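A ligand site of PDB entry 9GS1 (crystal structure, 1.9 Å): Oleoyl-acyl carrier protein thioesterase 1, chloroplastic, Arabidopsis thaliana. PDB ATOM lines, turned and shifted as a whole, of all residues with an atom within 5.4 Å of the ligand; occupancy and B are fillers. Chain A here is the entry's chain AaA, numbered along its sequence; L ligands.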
ATOM      1  N   LEU A  37     -21.299 -14.434  16.243  1.00  0.00           N
ATOM      2  CA  LEU A  37     -21.995 -14.084  17.524  1.00  0.00           C
ATOM      3  C   LEU A  37     -21.452 -14.980  18.640  1.00  0.00           C
ATOM      4  O   LEU A  37     -21.087 -14.506  19.702  1.00  0.00           O
ATOM      5  CB  LEU A  37     -23.514 -14.284  17.366  1.00  0.00           C
ATOM      6  CG  LEU A  37     -24.252 -13.424  16.340  1.00  0.00           C
ATOM      7  CD1 LEU A  37     -25.753 -13.638  16.431  1.00  0.00           C
ATOM      8  CD2 LEU A  37     -23.918 -11.949  16.498  1.00  0.00           C
ATOM      9  N   GLN A  38     -21.335 -16.285  18.372  1.00  0.00           N
ATOM     10  CA  GLN A  38     -20.876 -17.234  19.412  1.00  0.00           C
ATOM     11  C   GLN A  38     -19.420 -16.911  19.744  1.00  0.00           C
ATOM     12  O   GLN A  38     -19.055 -16.974  20.919  1.00  0.00           O
ATOM     13  CB  GLN A  38     -21.059 -18.674  18.944  1.00  0.00           C
ATOM     14  CG  GLN A  38     -20.919 -19.704  20.048  1.00  0.00           C
ATOM     15  CD  GLN A  38     -21.869 -20.860  19.788  1.00  0.00           C
ATOM     16  OE1 GLN A  38     -22.943 -20.998  20.395  1.00  0.00           O
ATOM     17  NE2 GLN A  38     -21.494 -21.684  18.835  1.00  0.00           N
ATOM     18  N   GLY A  41     -19.102 -13.863  21.885  1.00  0.00           N
ATOM     19  CA  GLY A  41     -19.565 -14.320  23.216  1.00  0.00           C
ATOM     20  C   GLY A  41     -18.522 -15.119  23.978  1.00  0.00           C
ATOM     21  O   GLY A  41     -18.279 -14.843  25.192  1.00  0.00           O
ATOM     22  N   CYS A  42     -17.916 -16.108  23.317  1.00  0.00           N
ATOM     23  CA  CYS A  42     -16.826 -16.921  23.918  1.00  0.00           C
ATOM     24  C   CYS A  42     -15.641 -16.015  24.283  1.00  0.00           C
ATOM     25  O   CYS A  42     -15.072 -16.228  25.400  1.00  0.00           O
ATOM     26  CB  CYS A  42     -16.411 -18.048  22.972  1.00  0.00           C
ATOM     27  SG  CYS A  42     -17.667 -19.345  22.796  1.00  0.00           S
ATOM     28  N   HIS A  44     -15.631 -12.782  24.972  1.00  0.00           N
ATOM     29  CA  HIS A  44     -16.080 -11.995  26.140  1.00  0.00           C
ATOM     30  C   HIS A  44     -15.812 -12.843  27.379  1.00  0.00           C
ATOM     31  O   HIS A  44     -15.117 -12.350  28.290  1.00  0.00           O
ATOM     32  CB  HIS A  44     -17.550 -11.563  25.977  1.00  0.00           C
ATOM     33  CG  HIS A  44     -18.007 -10.616  27.025  1.00  0.00           C
ATOM     34  ND1 HIS A  44     -19.321 -10.142  27.094  1.00  0.00           N
ATOM     35  CD2 HIS A  44     -17.357 -10.051  28.079  1.00  0.00           C
ATOM     36  CE1 HIS A  44     -19.448  -9.331  28.117  1.00  0.00           C
ATOM     37  NE2 HIS A  44     -18.276  -9.268  28.750  1.00  0.00           N
ATOM     38  N   ALA A  45     -16.326 -14.059  27.433  1.00  0.00           N
ATOM     39  CA  ALA A  45     -16.172 -14.980  28.589  1.00  0.00           C
ATOM     40  C   ALA A  45     -14.696 -15.098  28.959  1.00  0.00           C
ATOM     41  O   ALA A  45     -14.391 -15.042  30.154  1.00  0.00           O
ATOM     42  CB  ALA A  45     -16.747 -16.338  28.298  1.00  0.00           C
ATOM     43  N   VAL A  48     -13.003 -12.025  30.682  1.00  0.00           N
ATOM     44  CA  VAL A  48     -13.274 -11.785  32.136  1.00  0.00           C
ATOM     45  C   VAL A  48     -12.873 -13.001  32.975  1.00  0.00           C
ATOM     46  O   VAL A  48     -13.204 -12.990  34.163  1.00  0.00           O
ATOM     47  CB  VAL A  48     -14.736 -11.365  32.422  1.00  0.00           C
ATOM     48  CG1 VAL A  48     -15.033 -10.012  31.807  1.00  0.00           C
ATOM     49  CG2 VAL A  48     -15.741 -12.407  31.974  1.00  0.00           C
ATOM     50  N   PHE A  50     -13.275 -16.668  32.475  1.00  0.00           N
ATOM     51  CA  PHE A  50     -13.965 -17.978  32.521  1.00  0.00           C
ATOM     52  C   PHE A  50     -13.102 -18.971  31.755  1.00  0.00           C
ATOM     53  O   PHE A  50     -12.497 -18.551  30.747  1.00  0.00           O
ATOM     54  CB  PHE A  50     -15.409 -17.881  31.990  1.00  0.00           C
ATOM     55  CG  PHE A  50     -16.325 -17.159  32.923  1.00  0.00           C
ATOM     56  CD1 PHE A  50     -16.771 -17.759  34.087  1.00  0.00           C
ATOM     57  CD2 PHE A  50     -16.660 -15.832  32.707  1.00  0.00           C
ATOM     58  CE1 PHE A  50     -17.585 -17.064  34.977  1.00  0.00           C
ATOM     59  CE2 PHE A  50     -17.480 -15.138  33.590  1.00  0.00           C
ATOM     60  CZ  PHE A  50     -17.920 -15.758  34.739  1.00  0.00           C
ATOM     61  N   GLY A  54     -15.949 -25.090  29.081  1.00  0.00           N
ATOM     62  CA  GLY A  54     -17.355 -24.988  28.652  1.00  0.00           C
ATOM     63  C   GLY A  54     -17.703 -23.563  28.227  1.00  0.00           C
ATOM     64  O   GLY A  54     -16.763 -22.783  28.011  1.00  0.00           O
ATOM     65  N   PHE A  55     -19.006 -23.276  28.078  1.00  0.00           N
ATOM     66  CA  PHE A  55     -19.555 -21.909  27.892  1.00  0.00           C
ATOM     67  C   PHE A  55     -19.730 -21.216  29.254  1.00  0.00           C
ATOM     68  O   PHE A  55     -20.816 -21.322  29.806  1.00  0.00           O
ATOM     69  CB  PHE A  55     -20.897 -21.944  27.156  1.00  0.00           C
ATOM     70  CG  PHE A  55     -20.780 -21.912  25.654  1.00  0.00           C
ATOM     71  CD1 PHE A  55     -19.800 -22.640  25.008  1.00  0.00           C
ATOM     72  CD2 PHE A  55     -21.631 -21.121  24.901  1.00  0.00           C
ATOM     73  CE1 PHE A  55     -19.696 -22.597  23.625  1.00  0.00           C
ATOM     74  CE2 PHE A  55     -21.516 -21.089  23.523  1.00  0.00           C
ATOM     75  CZ  PHE A  55     -20.552 -21.833  22.884  1.00  0.00           C
ATOM     76  N   ALA A  56     -18.692 -20.523  29.731  1.00  0.00           N
ATOM     77  CA  ALA A  56     -18.750 -19.664  30.939  1.00  0.00           C
ATOM     78  C   ALA A  56     -19.349 -20.474  32.095  1.00  0.00           C
ATOM     79  O   ALA A  56     -20.257 -20.018  32.807  1.00  0.00           O
ATOM     80  CB  ALA A  56     -19.536 -18.415  30.643  1.00  0.00           C
ATOM     81  N   THR A  58     -19.166 -21.459  35.634  1.00  0.00           N
ATOM     82  CA  THR A  58     -18.596 -20.843  36.870  1.00  0.00           C
ATOM     83  C   THR A  58     -18.023 -21.962  37.747  1.00  0.00           C
ATOM     84  O   THR A  58     -18.416 -23.126  37.567  1.00  0.00           O
ATOM     85  CB  THR A  58     -19.634 -19.999  37.630  1.00  0.00           C
ATOM     86  OG1 THR A  58     -20.491 -20.839  38.393  1.00  0.00           O
ATOM     87  CG2 THR A  58     -20.439 -19.112  36.712  1.00  0.00           C
ATOM     88  N   TRP A  68     -24.480 -24.162  30.984  1.00  0.00           N
ATOM     89  CA  TRP A  68     -25.414 -23.255  30.258  1.00  0.00           C
ATOM     90  C   TRP A  68     -25.796 -23.935  28.954  1.00  0.00           C
ATOM     91  O   TRP A  68     -24.892 -24.408  28.249  1.00  0.00           O
ATOM     92  CB  TRP A  68     -24.745 -21.908  30.014  1.00  0.00           C
ATOM     93  CG  TRP A  68     -24.430 -21.134  31.255  1.00  0.00           C
ATOM     94  CD1 TRP A  68     -23.192 -20.845  31.750  1.00  0.00           C
ATOM     95  CD2 TRP A  68     -25.378 -20.498  32.131  1.00  0.00           C
ATOM     96  NE1 TRP A  68     -23.312 -20.092  32.894  1.00  0.00           N
ATOM     97  CE2 TRP A  68     -24.638 -19.873  33.157  1.00  0.00           C
ATOM     98  CE3 TRP A  68     -26.761 -20.366  32.126  1.00  0.00           C
ATOM     99  CZ2 TRP A  68     -25.260 -19.137  34.165  1.00  0.00           C
ATOM    100  CZ3 TRP A  68     -27.382 -19.670  33.145  1.00  0.00           C
ATOM    101  CH2 TRP A  68     -26.629 -19.076  34.155  1.00  0.00           C
ATOM    102  N   CYS A  93     -23.987  -9.662  28.456  1.00  0.00           N
ATOM    103  CA  CYS A  93     -24.790 -10.706  29.105  1.00  0.00           C
ATOM    104  C   CYS A  93     -25.517 -10.061  30.288  1.00  0.00           C
ATOM    105  O   CYS A  93     -24.888  -9.240  31.014  1.00  0.00           O
ATOM    106  CB  CYS A  93     -23.896 -11.842  29.575  1.00  0.00           C
ATOM    107  SG  CYS A  93     -24.810 -13.228  30.256  1.00  0.00           S
ATOM    108  N   THR A 101     -29.539 -16.697  31.939  1.00  0.00           N
ATOM    109  CA  THR A 101     -28.838 -15.494  31.459  1.00  0.00           C
ATOM    110  C   THR A 101     -29.346 -15.202  30.045  1.00  0.00           C
ATOM    111  O   THR A 101     -29.945 -16.099  29.410  1.00  0.00           O
ATOM    112  CB  THR A 101     -27.313 -15.652  31.563  1.00  0.00           C
ATOM    113  OG1 THR A 101     -27.041 -16.928  30.996  1.00  0.00           O
ATOM    114  CG2 THR A 101     -26.804 -15.571  32.993  1.00  0.00           C
ATOM    115  N   ARG A 102     -29.113 -13.974  29.608  1.00  0.00           N
ATOM    116  CA  ARG A 102     -29.492 -13.483  28.269  1.00  0.00           C
ATOM    117  C   ARG A 102     -28.246 -12.844  27.709  1.00  0.00           C
ATOM    118  O   ARG A 102     -27.683 -11.953  28.391  1.00  0.00           O
ATOM    119  CB  ARG A 102     -30.654 -12.486  28.327  1.00  0.00           C
ATOM    120  CG  ARG A 102     -31.239 -12.195  26.955  1.00  0.00           C
ATOM    121  CD  ARG A 102     -32.342 -11.145  26.931  1.00  0.00           C
ATOM    122  NE  ARG A 102     -31.696  -9.858  27.041  1.00  0.00           N
ATOM    123  CZ  ARG A 102     -31.558  -9.108  28.133  1.00  0.00           C
ATOM    124  NH1 ARG A 102     -30.850  -7.987  28.042  1.00  0.00           N
ATOM    125  NH2 ARG A 102     -32.080  -9.453  29.291  1.00  0.00           N
ATOM    126  N   ARG A 103     -27.804 -13.281  26.529  1.00  0.00           N
ATOM    127  CA  ARG A 103     -26.708 -12.606  25.818  1.00  0.00           C
ATOM    128  C   ARG A 103     -27.300 -11.922  24.602  1.00  0.00           C
ATOM    129  O   ARG A 103     -28.031 -12.546  23.856  1.00  0.00           O
ATOM    130  CB  ARG A 103     -25.557 -13.554  25.440  1.00  0.00           C
ATOM    131  CG  ARG A 103     -24.484 -12.882  24.613  1.00  0.00           C
ATOM    132  CD  ARG A 103     -23.173 -13.657  24.564  1.00  0.00           C
ATOM    133  NE  ARG A 103     -22.452 -13.689  25.850  1.00  0.00           N
ATOM    134  CZ  ARG A 103     -21.645 -12.725  26.320  1.00  0.00           C
ATOM    135  NH1 ARG A 103     -21.033 -12.878  27.490  1.00  0.00           N
ATOM    136  NH2 ARG A 103     -21.470 -11.612  25.651  1.00  0.00           N
ATOM    137  N   TRP A 105     -26.448  -9.030  21.249  1.00  0.00           N
ATOM    138  CA  TRP A 105     -25.446  -8.568  20.271  1.00  0.00           C
ATOM    139  C   TRP A 105     -26.026  -7.409  19.430  1.00  0.00           C
ATOM    140  O   TRP A 105     -27.227  -7.448  19.064  1.00  0.00           O
ATOM    141  CB  TRP A 105     -24.978  -9.713  19.354  1.00  0.00           C
ATOM    142  CG  TRP A 105     -24.341 -10.928  19.967  1.00  0.00           C
ATOM    143  CD1 TRP A 105     -23.004 -11.225  20.006  1.00  0.00           C
ATOM    144  CD2 TRP A 105     -24.998 -12.118  20.444  1.00  0.00           C
ATOM    145  NE1 TRP A 105     -22.795 -12.486  20.495  1.00  0.00           N
ATOM    146  CE2 TRP A 105     -23.992 -13.049  20.797  1.00  0.00           C
ATOM    147  CE3 TRP A 105     -26.335 -12.488  20.625  1.00  0.00           C
ATOM    148  CZ2 TRP A 105     -24.288 -14.314  21.300  1.00  0.00           C
ATOM    149  CZ3 TRP A 105     -26.630 -13.723  21.147  1.00  0.00           C
ATOM    150  CH2 TRP A 105     -25.610 -14.627  21.464  1.00  0.00           C
ATOM    151  N   TRP A 123     -30.358 -18.354  27.718  1.00  0.00           N
ATOM    152  CA  TRP A 123     -29.588 -19.535  28.162  1.00  0.00           C
ATOM    153  C   TRP A 123     -30.093 -19.930  29.539  1.00  0.00           C
ATOM    154  O   TRP A 123     -30.415 -19.042  30.358  1.00  0.00           O
ATOM    155  CB  TRP A 123     -28.098 -19.231  28.192  1.00  0.00           C
ATOM    156  CG  TRP A 123     -27.504 -18.893  26.847  1.00  0.00           C
ATOM    157  CD1 TRP A 123     -27.678 -17.746  26.140  1.00  0.00           C
ATOM    158  CD2 TRP A 123     -26.633 -19.716  26.066  1.00  0.00           C
ATOM    159  NE1 TRP A 123     -26.959 -17.795  24.972  1.00  0.00           N
ATOM    160  CE2 TRP A 123     -26.301 -18.995  24.902  1.00  0.00           C
ATOM    161  CE3 TRP A 123     -26.072 -20.990  26.242  1.00  0.00           C
ATOM    162  CZ2 TRP A 123     -25.452 -19.498  23.912  1.00  0.00           C
ATOM    163  CZ3 TRP A 123     -25.230 -21.483  25.270  1.00  0.00           C
ATOM    164  CH2 TRP A 123     -24.934 -20.756  24.108  1.00  0.00           C
ATOM    165  N   TYR A 144     -20.909 -14.494  38.604  1.00  0.00           N
ATOM    166  CA  TYR A 144     -20.876 -13.789  37.287  1.00  0.00           C
ATOM    167  C   TYR A 144     -21.540 -12.404  37.295  1.00  0.00           C
ATOM    168  O   TYR A 144     -21.317 -11.699  36.302  1.00  0.00           O
ATOM    169  CB  TYR A 144     -21.458 -14.668  36.178  1.00  0.00           C
ATOM    170  CG  TYR A 144     -22.933 -14.881  36.231  1.00  0.00           C
ATOM    171  CD1 TYR A 144     -23.822 -13.932  35.769  1.00  0.00           C
ATOM    172  CD2 TYR A 144     -23.473 -16.058  36.710  1.00  0.00           C
ATOM    173  CE1 TYR A 144     -25.187 -14.119  35.826  1.00  0.00           C
ATOM    174  CE2 TYR A 144     -24.840 -16.270  36.762  1.00  0.00           C
ATOM    175  CZ  TYR A 144     -25.707 -15.296  36.313  1.00  0.00           C
ATOM    176  OH  TYR A 144     -27.054 -15.501  36.387  1.00  0.00           O
ATOM    177  N   PHE A 147     -19.979  -9.034  36.070  1.00  0.00           N
ATOM    178  CA  PHE A 147     -19.590  -8.928  34.645  1.00  0.00           C
ATOM    179  C   PHE A 147     -20.785  -8.446  33.807  1.00  0.00           C
ATOM    180  O   PHE A 147     -20.564  -8.221  32.582  1.00  0.00           O
ATOM    181  CB  PHE A 147     -19.008 -10.258  34.131  1.00  0.00           C
ATOM    182  CG  PHE A 147     -17.767 -10.691  34.872  1.00  0.00           C
ATOM    183  CD1 PHE A 147     -16.697  -9.827  35.023  1.00  0.00           C
ATOM    184  CD2 PHE A 147     -17.692 -11.933  35.475  1.00  0.00           C
ATOM    185  CE1 PHE A 147     -15.574 -10.194  35.741  1.00  0.00           C
ATOM    186  CE2 PHE A 147     -16.553 -12.299  36.178  1.00  0.00           C
ATOM    187  CZ  PHE A 147     -15.494 -11.429  36.311  1.00  0.00           C
ATOM    188  N   CYS A 148     -21.949  -8.306  34.429  1.00  0.00           N
ATOM    189  CA  CYS A 148     -23.233  -8.000  33.736  1.00  0.00           C
ATOM    190  C   CYS A 148     -23.678  -6.575  34.044  1.00  0.00           C
ATOM    191  O   CYS A 148     -23.663  -6.176  35.195  1.00  0.00           O
ATOM    192  CB  CYS A 148     -24.346  -8.942  34.139  1.00  0.00           C
ATOM    193  SG  CYS A 148     -23.921 -10.698  33.903  1.00  0.00           S
HETATM  194  C1  LIG L   1     -20.359 -18.081  26.283  1.00  0.00           C
HETATM  195  C2  LIG L   1     -20.735 -17.779  24.968  1.00  0.00           C
HETATM  196  C3  LIG L   1     -22.018 -17.356  24.735  1.00  0.00           C
HETATM  197  C4  LIG L   1     -22.937 -17.250  25.778  1.00  0.00           C
HETATM  198  C5  LIG L   1     -24.132 -18.852  28.479  1.00  0.00           C
HETATM  199  C6  LIG L   1     -22.558 -17.533  27.086  1.00  0.00           C
HETATM  200  C7  LIG L   1     -24.753 -16.582  27.852  1.00  0.00           C
HETATM  201  C8  LIG L   1     -23.585 -17.435  28.242  1.00  0.00           C
HETATM  202  C9  LIG L   1     -23.574 -17.427  30.731  1.00  0.00           C
HETATM  203  C10 LIG L   1     -22.211 -15.843  29.452  1.00  0.00           C
HETATM  204  N1  LIG L   1     -22.994 -16.914  29.500  1.00  0.00           N
HETATM  205  C11 LIG L   1     -21.591 -15.489  30.718  1.00  0.00           C
HETATM  206  O1  LIG L   1     -22.593 -17.356  31.754  1.00  0.00           O
HETATM  207  O2  LIG L   1     -22.109 -15.163  28.478  1.00  0.00           O
HETATM  208  C12 LIG L   1     -21.759 -16.278  31.768  1.00  0.00           C
HETATM  209  C13 LIG L   1     -21.043 -16.158  33.070  1.00  0.00           C
HETATM  210 CL1  LIG L   1     -18.740 -18.653  26.614  1.00  0.00          CL
HETATM  211 CL2  LIG L   1     -22.552 -17.040  23.091  1.00  0.00          CL
HETATM  212  C14 LIG L   1     -21.264 -17.962  27.337  1.00  0.00           C
HETATM  213  C15 LIG L   1     -20.848 -14.195  30.807  1.00  0.00           C
HETATM  214  C16 LIG L   1     -21.389 -13.132  31.485  1.00  0.00           C
HETATM  215  C17 LIG L   1     -20.705 -11.925  31.555  1.00  0.00           C
HETATM  216  C18 LIG L   1     -19.492 -11.771  30.888  1.00  0.00           C
HETATM  217  C19 LIG L   1     -18.957 -12.823  30.158  1.00  0.00           C
HETATM  218  C20 LIG L   1     -19.621 -14.043  30.142  1.00  0.00           C
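SG of Cys 93 sits close to O2 of the ligand (3.8 Å).
The indole nitrogen (NE1) of Trp 68 is in hydrogen-bond range of an oxygen (O1) of the ligand (3.0 Å).
The guanidinium group (NH1) of Arg 103 sits at hydrogen-bond distance from an oxygen (O2) of the ligand (2.7 Å).
The backbone carbonyl oxygen (O) of Gln 38 sits at hydrogen-bond distance from the side-chain sulfur (SG) of Cys 42 (3.3 Å).
NH2 of Arg 103 lies within hydrogen-bond range of ND1 of His 44, 3.0 Å away.
The backbone carbonyl oxygen of Thr 101 is in hydrogen-bond range of the backbone NH of Trp 123 (2.8 Å).
The backbone NH (N) of Phe 50 lies within hydrogen-bond range of the backbone carbonyl oxygen (O) of Ala 45 (3.0 Å).
O of Ala 56 sits at hydrogen-bond distance from NE1 of Trp 68, at 3.1 Å.
O of Tyr 144 sits at hydrogen-bond distance from SG of Cys 148 (3.7 Å).
The side-chain sulfur of Cys 148 lies close to the backbone carbonyl oxygen of Cys 93 (3.4 Å).
NE1 of Trp 105 lies within hydrogen-bond range of O of Leu 37 (2.8 Å).
Residues that only touch the ligand: Gly 41 (3.6 Å), Cys 42 (3.7 Å), His 44 (3.5 Å), Ala 45 (3.5 Å), Val 48 (3.7 Å), Phe 50 (3.6 Å), Phe 55 (3.5 Å), Ala 56 (3.3 Å), Thr 101 (3.5 Å), Trp 105 (3.7 Å), Trp 123 (3.6 Å), Tyr 144 (3.5 Å) and Phe 147 (3.5 Å).
16 residues have an atom within 4 Å of the ligand: Gly 41, Cys 42, His 44, Ala 45, Val 48, Phe 50, Phe 55, Ala 56, Trp 68, Cys 93, Thr 101, Arg 103, Trp 105, Trp 123, Tyr 144 and Phe 147.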
